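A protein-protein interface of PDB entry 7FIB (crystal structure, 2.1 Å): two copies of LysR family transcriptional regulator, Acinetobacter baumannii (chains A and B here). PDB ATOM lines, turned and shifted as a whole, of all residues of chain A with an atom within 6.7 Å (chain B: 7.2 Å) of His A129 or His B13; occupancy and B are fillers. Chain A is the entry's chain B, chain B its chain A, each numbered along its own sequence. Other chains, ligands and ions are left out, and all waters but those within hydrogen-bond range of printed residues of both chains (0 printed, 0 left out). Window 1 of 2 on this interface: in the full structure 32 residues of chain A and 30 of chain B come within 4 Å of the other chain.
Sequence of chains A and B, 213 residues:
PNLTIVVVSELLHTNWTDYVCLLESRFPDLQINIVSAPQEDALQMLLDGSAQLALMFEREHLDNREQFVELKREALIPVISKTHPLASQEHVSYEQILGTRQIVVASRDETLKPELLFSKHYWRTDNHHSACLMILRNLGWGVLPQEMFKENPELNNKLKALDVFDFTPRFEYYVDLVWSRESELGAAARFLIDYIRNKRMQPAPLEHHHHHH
O of Leu B12 sits at hydrogen-bond distance from NE2 of His A129, at 3.4 Å.
A ring nitrogen (NE2) of His B13 lies close to a ring nitrogen (NE2) of His A129 (3.5 Å).
A ring nitrogen (NE2) of His B129 lies within hydrogen-bond range of a ring nitrogen (ND1) of His A13, 3.2 Å away.
Of the 24 printed residues of chain B, 5 touch a printed residue of chain A.
Of the 13 printed residues of chain A, 4 touch a printed residue of chain B.
Hydrophobic or aromatic side chains of chain A that line the printed part of chain B: His A13, His A129 and Leu A133.
Among the printed residues, 7 pairs touch across the chains.
The backbone carbonyl oxygen of Leu B12 sits at hydrogen-bond distance from the indole nitrogen of Trp B16 (2.9 Å).
The side-chain amide oxygen of Asn B127 sits at hydrogen-bond distance from the backbone NH of His B129.
OD1 of Asn A127 lies within hydrogen-bond range of N of His A129, 3.1 Å away.
The backbone NH (N) of Ser A130 lies within hydrogen-bond range of the side-chain amide oxygen (OD1) of Asn A127 (3.0 Å).
Among the printed residues, merely in contact across the chains: His A129 with Glu B151, Ser A130 with Trp B16, Leu A133 with Trp B16 and Leu A133 with Glu B151.
Of chain B, only Leu B12 (3.4 Å), His B13 (3.1 Å) and Glu B151 (3.6 Å) come within 4 Å of His A129.
His B13 touches one residue of chain A.
Printed residues of chain A within 4 Å of His B129: His A13 (3.2 Å).
Of the printed residues of chain B, Ser A130 touches Trp B16.
Of the printed residues of chain A, Glu B151 touches His A129 and Leu A133.
Of the printed residues of chain A, Leu B12 touches His A129 (3.4 Å).
Printed residues of chain A within 4 Å of Trp B16: Ser A130 (3.7 Å) and Leu A133 (3.7 Å).
Glu B147 touches none of the printed residues of chain A.
Cys A132 touches none of the printed residues of chain B.
The nearest residue of chain B that does not touch His A129 is Trp B16 (5.2 Å).
The nearest residue of chain A that does not touch His B13 is His A13 (5.7 Å).
His A13 touches His B129, and with the chains exchanged His A129 touches His B13.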
ATOM      1  N   HIS A  13      -8.681  33.755 -33.702  1.00  0.00           N
ATOM      2  CA  HIS A  13      -9.458  34.907 -33.227  1.00  0.00           C
ATOM      3  C   HIS A  13      -9.122  36.162 -34.029  1.00  0.00           C
ATOM      4  O   HIS A  13      -8.616  37.149 -33.509  1.00  0.00           O
ATOM      5  CB  HIS A  13      -9.230  35.126 -31.733  1.00  0.00           C
ATOM      6  CG  HIS A  13      -9.459  33.902 -30.901  1.00  0.00           C
ATOM      7  ND1 HIS A  13     -10.680  33.613 -30.328  1.00  0.00           N
ATOM      8  CD2 HIS A  13      -8.626  32.906 -30.524  1.00  0.00           C
ATOM      9  CE1 HIS A  13     -10.604  32.469 -29.671  1.00  0.00           C
ATOM     10  NE2 HIS A  13      -9.365  32.019 -29.770  1.00  0.00           N
ATOM     11  N   VAL A 105       1.279  31.286 -25.972  1.00  0.00           N
ATOM     12  CA  VAL A 105       0.713  30.460 -27.034  1.00  0.00           C
ATOM     13  C   VAL A 105       1.804  30.147 -28.058  1.00  0.00           C
ATOM     14  O   VAL A 105       2.471  31.055 -28.574  1.00  0.00           O
ATOM     15  CB  VAL A 105      -0.501  31.141 -27.692  1.00  0.00           C
ATOM     16  CG1 VAL A 105      -1.107  30.253 -28.790  1.00  0.00           C
ATOM     17  CG2 VAL A 105      -1.566  31.430 -26.653  1.00  0.00           C
ATOM     18  N   THR A 125       0.451  26.971 -23.990  1.00  0.00           N
ATOM     19  CA  THR A 125      -0.744  26.385 -24.543  1.00  0.00           C
ATOM     20  C   THR A 125      -0.716  26.641 -26.043  1.00  0.00           C
ATOM     21  O   THR A 125       0.152  27.356 -26.550  1.00  0.00           O
ATOM     22  CB  THR A 125      -1.989  26.946 -23.867  1.00  0.00           C
ATOM     23  OG1 THR A 125      -3.119  26.164 -24.250  1.00  0.00           O
ATOM     24  CG2 THR A 125      -2.216  28.405 -24.276  1.00  0.00           C
ATOM     25  N   ASN A 127      -3.486  27.648 -27.978  1.00  0.00           N
ATOM     26  CA  ASN A 127      -4.485  28.550 -28.538  1.00  0.00           C
ATOM     27  C   ASN A 127      -4.910  29.578 -27.491  1.00  0.00           C
ATOM     28  O   ASN A 127      -4.728  29.386 -26.286  1.00  0.00           O
ATOM     29  CB  ASN A 127      -5.686  27.772 -29.087  1.00  0.00           C
ATOM     30  CG  ASN A 127      -6.551  27.220 -27.995  1.00  0.00           C
ATOM     31  OD1 ASN A 127      -7.466  27.891 -27.529  1.00  0.00           O
ATOM     32  ND2 ASN A 127      -6.248  25.998 -27.554  1.00  0.00           N
ATOM     33  N   HIS A 128      -5.467  30.687 -27.982  1.00  0.00           N
ATOM     34  CA  HIS A 128      -5.724  31.845 -27.130  1.00  0.00           C
ATOM     35  C   HIS A 128      -6.944  31.653 -26.234  1.00  0.00           C
ATOM     36  O   HIS A 128      -7.032  32.262 -25.161  1.00  0.00           O
ATOM     37  CB  HIS A 128      -5.885  33.097 -27.985  1.00  0.00           C
ATOM     38  CG  HIS A 128      -4.619  33.518 -28.653  1.00  0.00           C
ATOM     39  ND1 HIS A 128      -3.575  34.108 -27.964  1.00  0.00           N
ATOM     40  CD2 HIS A 128      -4.219  33.425 -29.936  1.00  0.00           C
ATOM     41  CE1 HIS A 128      -2.590  34.367 -28.803  1.00  0.00           C
ATOM     42  NE2 HIS A 128      -2.955  33.957 -30.004  1.00  0.00           N
ATOM     43  N   HIS A 129      -7.911  30.847 -26.662  1.00  0.00           N
ATOM     44  CA  HIS A 129      -9.024  30.534 -25.775  1.00  0.00           C
ATOM     45  C   HIS A 129      -8.522  29.862 -24.501  1.00  0.00           C
ATOM     46  O   HIS A 129      -8.867  30.277 -23.394  1.00  0.00           O
ATOM     47  CB  HIS A 129     -10.041  29.643 -26.486  1.00  0.00           C
ATOM     48  CG  HIS A 129     -11.090  29.082 -25.570  1.00  0.00           C
ATOM     49  ND1 HIS A 129     -12.063  29.867 -24.980  1.00  0.00           N
ATOM     50  CD2 HIS A 129     -11.325  27.816 -25.151  1.00  0.00           C
ATOM     51  CE1 HIS A 129     -12.846  29.106 -24.234  1.00  0.00           C
ATOM     52  NE2 HIS A 129     -12.427  27.857 -24.328  1.00  0.00           N
ATOM     53  N   SER A 130      -7.694  28.828 -24.646  1.00  0.00           N
ATOM     54  CA  SER A 130      -7.123  28.165 -23.480  1.00  0.00           C
ATOM     55  C   SER A 130      -6.304  29.136 -22.637  1.00  0.00           C
ATOM     56  O   SER A 130      -6.433  29.158 -21.408  1.00  0.00           O
ATOM     57  CB  SER A 130      -6.262  26.983 -23.915  1.00  0.00           C
ATOM     58  OG  SER A 130      -7.068  25.989 -24.512  1.00  0.00           O
ATOM     59  N   ALA A 131      -5.466  29.955 -23.280  1.00  0.00           N
ATOM     60  CA  ALA A 131      -4.703  30.956 -22.543  1.00  0.00           C
ATOM     61  C   ALA A 131      -5.630  31.877 -21.763  1.00  0.00           C
ATOM     62  O   ALA A 131      -5.426  32.119 -20.567  1.00  0.00           O
ATOM     63  CB  ALA A 131      -3.831  31.762 -23.524  1.00  0.00           C
ATOM     64  N   CYS A 132      -6.666  32.393 -22.433  1.00  0.00           N
ATOM     65  CA  CYS A 132      -7.619  33.286 -21.789  1.00  0.00           C
ATOM     66  C   CYS A 132      -8.248  32.642 -20.558  1.00  0.00           C
ATOM     67  O   CYS A 132      -8.309  33.260 -19.487  1.00  0.00           O
ATOM     68  CB  CYS A 132      -8.701  33.675 -22.806  1.00  0.00           C
ATOM     69  SG  CYS A 132      -9.809  35.006 -22.242  1.00  0.00           S
ATOM     70  N   LEU A 133      -8.729  31.399 -20.688  1.00  0.00           N
ATOM     71  CA  LEU A 133      -9.391  30.772 -19.555  1.00  0.00           C
ATOM     72  C   LEU A 133      -8.482  30.738 -18.336  1.00  0.00           C
ATOM     73  O   LEU A 133      -8.920  31.033 -17.219  1.00  0.00           O
ATOM     74  CB  LEU A 133      -9.844  29.364 -19.918  1.00  0.00           C
ATOM     75  CG  LEU A 133     -11.103  29.265 -20.785  1.00  0.00           C
ATOM     76  CD1 LEU A 133     -11.526  27.820 -20.869  1.00  0.00           C
ATOM     77  CD2 LEU A 133     -12.217  30.092 -20.197  1.00  0.00           C
ATOM     78  N   MET A 134      -7.206  30.404 -18.529  1.00  0.00           N
ATOM     79  CA  MET A 134      -6.303  30.299 -17.389  1.00  0.00           C
ATOM     80  C   MET A 134      -5.967  31.660 -16.793  1.00  0.00           C
ATOM     81  O   MET A 134      -5.846  31.787 -15.561  1.00  0.00           O
ATOM     82  CB  MET A 134      -5.045  29.533 -17.797  1.00  0.00           C
ATOM     83  CG  MET A 134      -5.362  28.063 -18.148  1.00  0.00           C
ATOM     84  SD  MET A 134      -3.961  27.014 -18.445  1.00  0.00           S
ATOM     85  CE  MET A 134      -3.629  27.289 -20.204  1.00  0.00           C
ATOM     86  N   LEU A 144      -3.193  38.491 -25.552  1.00  0.00           N
ATOM     87  CA  LEU A 144      -4.387  38.030 -26.240  1.00  0.00           C
ATOM     88  C   LEU A 144      -4.752  38.914 -27.429  1.00  0.00           C
ATOM     89  O   LEU A 144      -4.532  40.127 -27.411  1.00  0.00           O
ATOM     90  CB  LEU A 144      -5.584  37.971 -25.288  1.00  0.00           C
ATOM     91  CG  LEU A 144      -5.549  37.095 -24.032  1.00  0.00           C
ATOM     92  CD1 LEU A 144      -6.884  37.205 -23.330  1.00  0.00           C
ATOM     93  CD2 LEU A 144      -5.264  35.645 -24.384  1.00  0.00           C
ATOM     94  N   MET A 148     -10.517  39.414 -29.271  1.00  0.00           N
ATOM     95  CA  MET A 148     -11.285  38.654 -28.282  1.00  0.00           C
ATOM     96  C   MET A 148     -12.139  39.570 -27.416  1.00  0.00           C
ATOM     97  O   MET A 148     -13.196  39.164 -26.918  1.00  0.00           O
ATOM     98  CB  MET A 148     -10.362  37.809 -27.401  1.00  0.00           C
ATOM     99  CG  MET A 148      -9.586  36.722 -28.132  1.00  0.00           C
ATOM    100  SD  MET A 148      -8.812  35.563 -26.943  1.00  0.00           S
ATOM    101  CE  MET A 148     -10.228  34.915 -26.054  1.00  0.00           C
ATOM    102  N   VAL B   7      -6.448  18.273 -24.334  1.00  0.00           N
ATOM    103  CA  VAL B   7      -7.899  18.391 -24.284  1.00  0.00           C
ATOM    104  C   VAL B   7      -8.410  18.210 -25.701  1.00  0.00           C
ATOM    105  O   VAL B   7      -8.070  18.995 -26.591  1.00  0.00           O
ATOM    106  CB  VAL B   7      -8.333  19.741 -23.701  1.00  0.00           C
ATOM    107  CG1 VAL B   7      -9.851  19.912 -23.766  1.00  0.00           C
ATOM    108  CG2 VAL B   7      -7.790  19.907 -22.285  1.00  0.00           C
ATOM    109  N   VAL B   8      -9.165  17.132 -25.933  1.00  0.00           N
ATOM    110  CA  VAL B   8      -9.701  16.877 -27.265  1.00  0.00           C
ATOM    111  C   VAL B   8     -10.471  18.107 -27.758  1.00  0.00           C
ATOM    112  O   VAL B   8     -11.151  18.786 -26.990  1.00  0.00           O
ATOM    113  CB  VAL B   8     -10.562  15.601 -27.224  1.00  0.00           C
ATOM    114  CG1 VAL B   8     -11.541  15.535 -28.363  1.00  0.00           C
ATOM    115  CG2 VAL B   8      -9.645  14.375 -27.254  1.00  0.00           C
ATOM    116  N   SER B   9     -10.350  18.398 -29.061  1.00  0.00           N
ATOM    117  CA  SER B   9     -10.867  19.661 -29.595  1.00  0.00           C
ATOM    118  C   SER B   9     -12.311  19.929 -29.169  1.00  0.00           C
ATOM    119  O   SER B   9     -12.642  21.054 -28.767  1.00  0.00           O
ATOM    120  CB  SER B   9     -10.746  19.679 -31.126  1.00  0.00           C
ATOM    121  OG  SER B   9      -9.392  19.503 -31.541  1.00  0.00           O
ATOM    122  N   GLU B  10     -13.177  18.902 -29.223  1.00  0.00           N
ATOM    123  CA  GLU B  10     -14.608  19.094 -28.945  1.00  0.00           C
ATOM    124  C   GLU B  10     -14.878  19.570 -27.524  1.00  0.00           C
ATOM    125  O   GLU B  10     -15.968  20.094 -27.246  1.00  0.00           O
ATOM    126  CB  GLU B  10     -15.369  17.796 -29.188  1.00  0.00           C
ATOM    127  CG  GLU B  10     -15.628  17.518 -30.640  1.00  0.00           C
ATOM    128  CD  GLU B  10     -14.447  16.839 -31.297  1.00  0.00           C
ATOM    129  OE1 GLU B  10     -13.372  16.707 -30.663  1.00  0.00           O
ATOM    130  OE2 GLU B  10     -14.603  16.422 -32.451  1.00  0.00           O
ATOM    131  N   LEU B  11     -13.924  19.364 -26.617  1.00  0.00           N
ATOM    132  CA  LEU B  11     -14.066  19.672 -25.202  1.00  0.00           C
ATOM    133  C   LEU B  11     -13.356  20.953 -24.804  1.00  0.00           C
ATOM    134  O   LEU B  11     -13.319  21.277 -23.621  1.00  0.00           O
ATOM    135  CB  LEU B  11     -13.536  18.498 -24.356  1.00  0.00           C
ATOM    136  CG  LEU B  11     -14.158  17.135 -24.685  1.00  0.00           C
ATOM    137  CD1 LEU B  11     -13.642  16.017 -23.757  1.00  0.00           C
ATOM    138  CD2 LEU B  11     -15.702  17.229 -24.656  1.00  0.00           C
ATOM    139  N   LEU B  12     -12.759  21.664 -25.758  1.00  0.00           N
ATOM    140  CA  LEU B  12     -12.054  22.904 -25.440  1.00  0.00           C
ATOM    141  C   LEU B  12     -12.961  23.903 -24.720  1.00  0.00           C
ATOM    142  O   LEU B  12     -12.571  24.505 -23.715  1.00  0.00           O
ATOM    143  CB  LEU B  12     -11.518  23.490 -26.738  1.00  0.00           C
ATOM    144  CG  LEU B  12     -10.464  22.808 -27.577  1.00  0.00           C
ATOM    145  CD1 LEU B  12     -10.226  23.527 -28.867  1.00  0.00           C
ATOM    146  CD2 LEU B  12      -9.183  22.739 -26.741  1.00  0.00           C
ATOM    147  N   HIS B  13     -14.166  24.106 -25.233  1.00  0.00           N
ATOM    148  CA  HIS B  13     -15.081  25.102 -24.673  1.00  0.00           C
ATOM    149  C   HIS B  13     -16.000  24.496 -23.630  1.00  0.00           C
ATOM    150  O   HIS B  13     -17.188  24.783 -23.613  1.00  0.00           O
ATOM    151  CB  HIS B  13     -15.860  25.769 -25.800  1.00  0.00           C
ATOM    152  CG  HIS B  13     -14.994  26.627 -26.660  1.00  0.00           C
ATOM    153  ND1 HIS B  13     -14.335  26.144 -27.776  1.00  0.00           N
ATOM    154  CD2 HIS B  13     -14.599  27.913 -26.519  1.00  0.00           C
ATOM    155  CE1 HIS B  13     -13.590  27.101 -28.298  1.00  0.00           C
ATOM    156  NE2 HIS B  13     -13.730  28.184 -27.550  1.00  0.00           N
ATOM    157  N   THR B  14     -15.383  23.698 -22.738  1.00  0.00           N
ATOM    158  CA  THR B  14     -15.918  22.900 -21.625  1.00  0.00           C
ATOM    159  C   THR B  14     -15.196  23.375 -20.349  1.00  0.00           C
ATOM    160  O   THR B  14     -14.754  24.521 -20.327  1.00  0.00           O
ATOM    161  CB  THR B  14     -15.748  21.400 -22.019  1.00  0.00           C
ATOM    162  OG1 THR B  14     -16.810  21.013 -22.908  1.00  0.00           O
ATOM    163  CG2 THR B  14     -15.649  20.364 -20.878  1.00  0.00           C
ATOM    164  N   ASN B  15     -15.013  22.556 -19.303  1.00  0.00           N
ATOM    165  CA  ASN B  15     -14.757  23.014 -17.940  1.00  0.00           C
ATOM    166  C   ASN B  15     -13.428  22.537 -17.346  1.00  0.00           C
ATOM    167  O   ASN B  15     -13.277  22.467 -16.118  1.00  0.00           O
ATOM    168  CB  ASN B  15     -15.909  22.558 -17.055  1.00  0.00           C
ATOM    169  CG  ASN B  15     -15.521  22.446 -15.618  1.00  0.00           C
ATOM    170  OD1 ASN B  15     -15.452  21.342 -15.063  1.00  0.00           O
ATOM    171  ND2 ASN B  15     -15.310  23.582 -14.979  1.00  0.00           N
ATOM    172  N   TRP B  16     -12.440  22.260 -18.174  1.00  0.00           N
ATOM    173  CA  TRP B  16     -11.230  21.629 -17.684  1.00  0.00           C
ATOM    174  C   TRP B  16     -10.436  22.495 -16.717  1.00  0.00           C
ATOM    175  O   TRP B  16      -9.515  21.996 -16.051  1.00  0.00           O
ATOM    176  CB  TRP B  16     -10.387  21.276 -18.880  1.00  0.00           C
ATOM    177  CG  TRP B  16     -10.304  22.395 -19.854  1.00  0.00           C
ATOM    178  CD1 TRP B  16     -11.152  22.657 -20.895  1.00  0.00           C
ATOM    179  CD2 TRP B  16      -9.316  23.415 -19.870  1.00  0.00           C
ATOM    180  NE1 TRP B  16     -10.724  23.768 -21.589  1.00  0.00           N
ATOM    181  CE2 TRP B  16      -9.598  24.251 -20.978  1.00  0.00           C
ATOM    182  CE3 TRP B  16      -8.200  23.693 -19.069  1.00  0.00           C
ATOM    183  CZ2 TRP B  16      -8.816  25.355 -21.295  1.00  0.00           C
ATOM    184  CZ3 TRP B  16      -7.414  24.777 -19.391  1.00  0.00           C
ATOM    185  CH2 TRP B  16      -7.728  25.601 -20.506  1.00  0.00           C
ATOM    186  N   GLU B  74     -21.162  17.154 -20.097  1.00  0.00           N
ATOM    187  CA  GLU B  74     -21.243  18.510 -20.632  1.00  0.00           C
ATOM    188  C   GLU B  74     -22.419  18.632 -21.585  1.00  0.00           C
ATOM    189  O   GLU B  74     -22.576  17.833 -22.512  1.00  0.00           O
ATOM    190  CB  GLU B  74     -19.934  18.952 -21.312  1.00  0.00           C
ATOM    191  CG  GLU B  74     -18.775  19.143 -20.284  1.00  0.00           C
ATOM    192  CD  GLU B  74     -18.730  20.541 -19.622  1.00  0.00           C
ATOM    193  OE1 GLU B  74     -19.487  21.459 -20.018  1.00  0.00           O
ATOM    194  OE2 GLU B  74     -17.905  20.734 -18.707  1.00  0.00           O
ATOM    195  N   ALA B  75     -23.233  19.643 -21.347  1.00  0.00           N
ATOM    196  CA  ALA B  75     -24.465  19.850 -22.078  1.00  0.00           C
ATOM    197  C   ALA B  75     -24.225  20.762 -23.274  1.00  0.00           C
ATOM    198  O   ALA B  75     -23.521  21.771 -23.163  1.00  0.00           O
ATOM    199  CB  ALA B  75     -25.514  20.464 -21.150  1.00  0.00           C
ATOM    200  N   LEU B  76     -24.839  20.409 -24.405  1.00  0.00           N
ATOM    201  CA  LEU B  76     -24.800  21.174 -25.650  1.00  0.00           C
ATOM    202  C   LEU B  76     -26.222  21.504 -26.090  1.00  0.00           C
ATOM    203  O   LEU B  76     -27.152  20.735 -25.828  1.00  0.00           O
ATOM    204  CB  LEU B  76     -24.109  20.371 -26.756  1.00  0.00           C
ATOM    205  CG  LEU B  76     -22.881  19.552 -26.354  1.00  0.00           C
ATOM    206  CD1 LEU B  76     -22.528  18.451 -27.359  1.00  0.00           C
ATOM    207  CD2 LEU B  76     -21.732  20.484 -26.192  1.00  0.00           C
ATOM    208  N   ASN B 127     -13.705  22.868 -34.238  1.00  0.00           N
ATOM    209  CA  ASN B 127     -13.821  23.401 -32.885  1.00  0.00           C
ATOM    210  C   ASN B 127     -15.020  24.328 -32.775  1.00  0.00           C
ATOM    211  O   ASN B 127     -15.512  24.862 -33.777  1.00  0.00           O
ATOM    212  CB  ASN B 127     -12.552  24.141 -32.447  1.00  0.00           C
ATOM    213  CG  ASN B 127     -12.511  25.555 -32.967  1.00  0.00           C
ATOM    214  OD1 ASN B 127     -13.011  26.483 -32.330  1.00  0.00           O
ATOM    215  ND2 ASN B 127     -11.914  25.726 -34.133  1.00  0.00           N
ATOM    216  N   HIS B 128     -15.488  24.513 -31.535  1.00  0.00           N
ATOM    217  CA  HIS B 128     -16.778  25.173 -31.335  1.00  0.00           C
ATOM    218  C   HIS B 128     -16.684  26.685 -31.463  1.00  0.00           C
ATOM    219  O   HIS B 128     -17.697  27.340 -31.737  1.00  0.00           O
ATOM    220  CB  HIS B 128     -17.359  24.794 -29.969  1.00  0.00           C
ATOM    221  CG  HIS B 128     -17.751  23.354 -29.870  1.00  0.00           C
ATOM    222  ND1 HIS B 128     -18.861  22.844 -30.512  1.00  0.00           N
ATOM    223  CD2 HIS B 128     -17.185  22.313 -29.220  1.00  0.00           C
ATOM    224  CE1 HIS B 128     -18.959  21.552 -30.260  1.00  0.00           C
ATOM    225  NE2 HIS B 128     -17.962  21.207 -29.466  1.00  0.00           N
ATOM    226  N   HIS B 129     -15.495  27.259 -31.271  1.00  0.00           N
ATOM    227  CA  HIS B 129     -15.338  28.694 -31.498  1.00  0.00           C
ATOM    228  C   HIS B 129     -15.511  29.043 -32.977  1.00  0.00           C
ATOM    229  O   HIS B 129     -16.235  29.990 -33.313  1.00  0.00           O
ATOM    230  CB  HIS B 129     -13.977  29.172 -30.964  1.00  0.00           C
ATOM    231  CG  HIS B 129     -13.590  30.546 -31.424  1.00  0.00           C
ATOM    232  ND1 HIS B 129     -14.118  31.693 -30.869  1.00  0.00           N
ATOM    233  CD2 HIS B 129     -12.730  30.957 -32.386  1.00  0.00           C
ATOM    234  CE1 HIS B 129     -13.596  32.751 -31.462  1.00  0.00           C
ATOM    235  NE2 HIS B 129     -12.748  32.333 -32.386  1.00  0.00           N
ATOM    236  N   SER B 130     -14.873  28.281 -33.875  1.00  0.00           N
ATOM    237  CA  SER B 130     -15.098  28.490 -35.308  1.00  0.00           C
ATOM    238  C   SER B 130     -16.562  28.290 -35.670  1.00  0.00           C
ATOM    239  O   SER B 130     -17.141  29.086 -36.421  1.00  0.00           O
ATOM    240  CB  SER B 130     -14.237  27.533 -36.140  1.00  0.00           C
ATOM    241  OG  SER B 130     -12.851  27.763 -35.928  1.00  0.00           O
ATOM    242  N   LEU B 144     -23.717  23.977 -29.869  1.00  0.00           N
ATOM    243  CA  LEU B 144     -22.675  24.610 -29.073  1.00  0.00           C
ATOM    244  C   LEU B 144     -22.769  24.193 -27.609  1.00  0.00           C
ATOM    245  O   LEU B 144     -23.861  23.922 -27.094  1.00  0.00           O
ATOM    246  CB  LEU B 144     -22.772  26.140 -29.149  1.00  0.00           C
ATOM    247  CG  LEU B 144     -22.694  26.785 -30.549  1.00  0.00           C
ATOM    248  CD1 LEU B 144     -22.705  28.312 -30.464  1.00  0.00           C
ATOM    249  CD2 LEU B 144     -21.476  26.277 -31.352  1.00  0.00           C
ATOM    250  N   PRO B 145     -21.636  24.151 -26.912  1.00  0.00           N
ATOM    251  CA  PRO B 145     -21.667  23.880 -25.464  1.00  0.00           C
ATOM    252  C   PRO B 145     -22.377  24.987 -24.703  1.00  0.00           C
ATOM    253  O   PRO B 145     -22.177  26.175 -24.977  1.00  0.00           O
ATOM    254  CB  PRO B 145     -20.181  23.797 -25.077  1.00  0.00           C
ATOM    255  CG  PRO B 145     -19.452  23.442 -26.367  1.00  0.00           C
ATOM    256  CD  PRO B 145     -20.266  24.142 -27.472  1.00  0.00           C
ATOM    257  N   GLN B 146     -23.227  24.578 -23.745  1.00  0.00           N
ATOM    258  CA  GLN B 146     -23.851  25.555 -22.855  1.00  0.00           C
ATOM    259  C   GLN B 146     -22.808  26.417 -22.165  1.00  0.00           C
ATOM    260  O   GLN B 146     -23.047  27.603 -21.911  1.00  0.00           O
ATOM    261  CB  GLN B 146     -24.724  24.842 -21.816  1.00  0.00           C
ATOM    262  N   GLU B 147     -21.640  25.843 -21.880  1.00  0.00           N
ATOM    263  CA  GLU B 147     -20.580  26.567 -21.195  1.00  0.00           C
ATOM    264  C   GLU B 147     -20.185  27.828 -21.947  1.00  0.00           C
ATOM    265  O   GLU B 147     -19.830  28.839 -21.319  1.00  0.00           O
ATOM    266  CB  GLU B 147     -19.386  25.632 -21.016  1.00  0.00           C
ATOM    267  CG  GLU B 147     -18.210  26.205 -20.231  1.00  0.00           C
ATOM    268  CD  GLU B 147     -18.497  26.302 -18.734  1.00  0.00           C
ATOM    269  OE1 GLU B 147     -19.406  25.590 -18.234  1.00  0.00           O
ATOM    270  OE2 GLU B 147     -17.811  27.104 -18.063  1.00  0.00           O
ATOM    271  N   MET B 148     -20.253  27.798 -23.287  1.00  0.00           N
ATOM    272  CA  MET B 148     -19.930  28.994 -24.054  1.00  0.00           C
ATOM    273  C   MET B 148     -20.811  30.159 -23.632  1.00  0.00           C
ATOM    274  O   MET B 148     -20.353  31.306 -23.576  1.00  0.00           O
ATOM    275  CB  MET B 148     -20.076  28.727 -25.559  1.00  0.00           C
ATOM    276  CG  MET B 148     -18.967  27.893 -26.183  1.00  0.00           C
ATOM    277  SD  MET B 148     -19.095  27.907 -27.987  1.00  0.00           S
ATOM    278  CE  MET B 148     -18.695  29.631 -28.308  1.00  0.00           C
ATOM    279  N   PHE B 149     -22.074  29.879 -23.301  1.00  0.00           N
ATOM    280  CA  PHE B 149     -22.979  30.926 -22.843  1.00  0.00           C
ATOM    281  C   PHE B 149     -22.587  31.450 -21.464  1.00  0.00           C
ATOM    282  O   PHE B 149     -22.797  32.632 -21.163  1.00  0.00           O
ATOM    283  CB  PHE B 149     -24.414  30.397 -22.849  1.00  0.00           C
ATOM    284  CG  PHE B 149     -24.998  30.363 -24.211  1.00  0.00           C
ATOM    285  CD1 PHE B 149     -25.606  31.486 -24.736  1.00  0.00           C
ATOM    286  CD2 PHE B 149     -24.870  29.238 -25.002  1.00  0.00           C
ATOM    287  CE1 PHE B 149     -26.101  31.477 -26.011  1.00  0.00           C
ATOM    288  CE2 PHE B 149     -25.364  29.219 -26.296  1.00  0.00           C
ATOM    289  CZ  PHE B 149     -25.986  30.340 -26.796  1.00  0.00           C
ATOM    290  N   GLU B 151     -19.335  31.497 -20.484  1.00  0.00           N
ATOM    291  CA  GLU B 151     -18.116  32.249 -20.776  1.00  0.00           C
ATOM    292  C   GLU B 151     -18.421  33.614 -21.395  1.00  0.00           C
ATOM    293  O   GLU B 151     -17.681  34.578 -21.182  1.00  0.00           O
ATOM    294  CB  GLU B 151     -17.217  31.419 -21.700  1.00  0.00           C
ATOM    295  CG  GLU B 151     -16.443  30.301 -20.994  1.00  0.00           C
ATOM    296  CD  GLU B 151     -16.023  29.144 -21.919  1.00  0.00           C
ATOM    297  OE1 GLU B 151     -16.265  29.211 -23.155  1.00  0.00           O
ATOM    298  OE2 GLU B 151     -15.457  28.149 -21.394  1.00  0.00           O
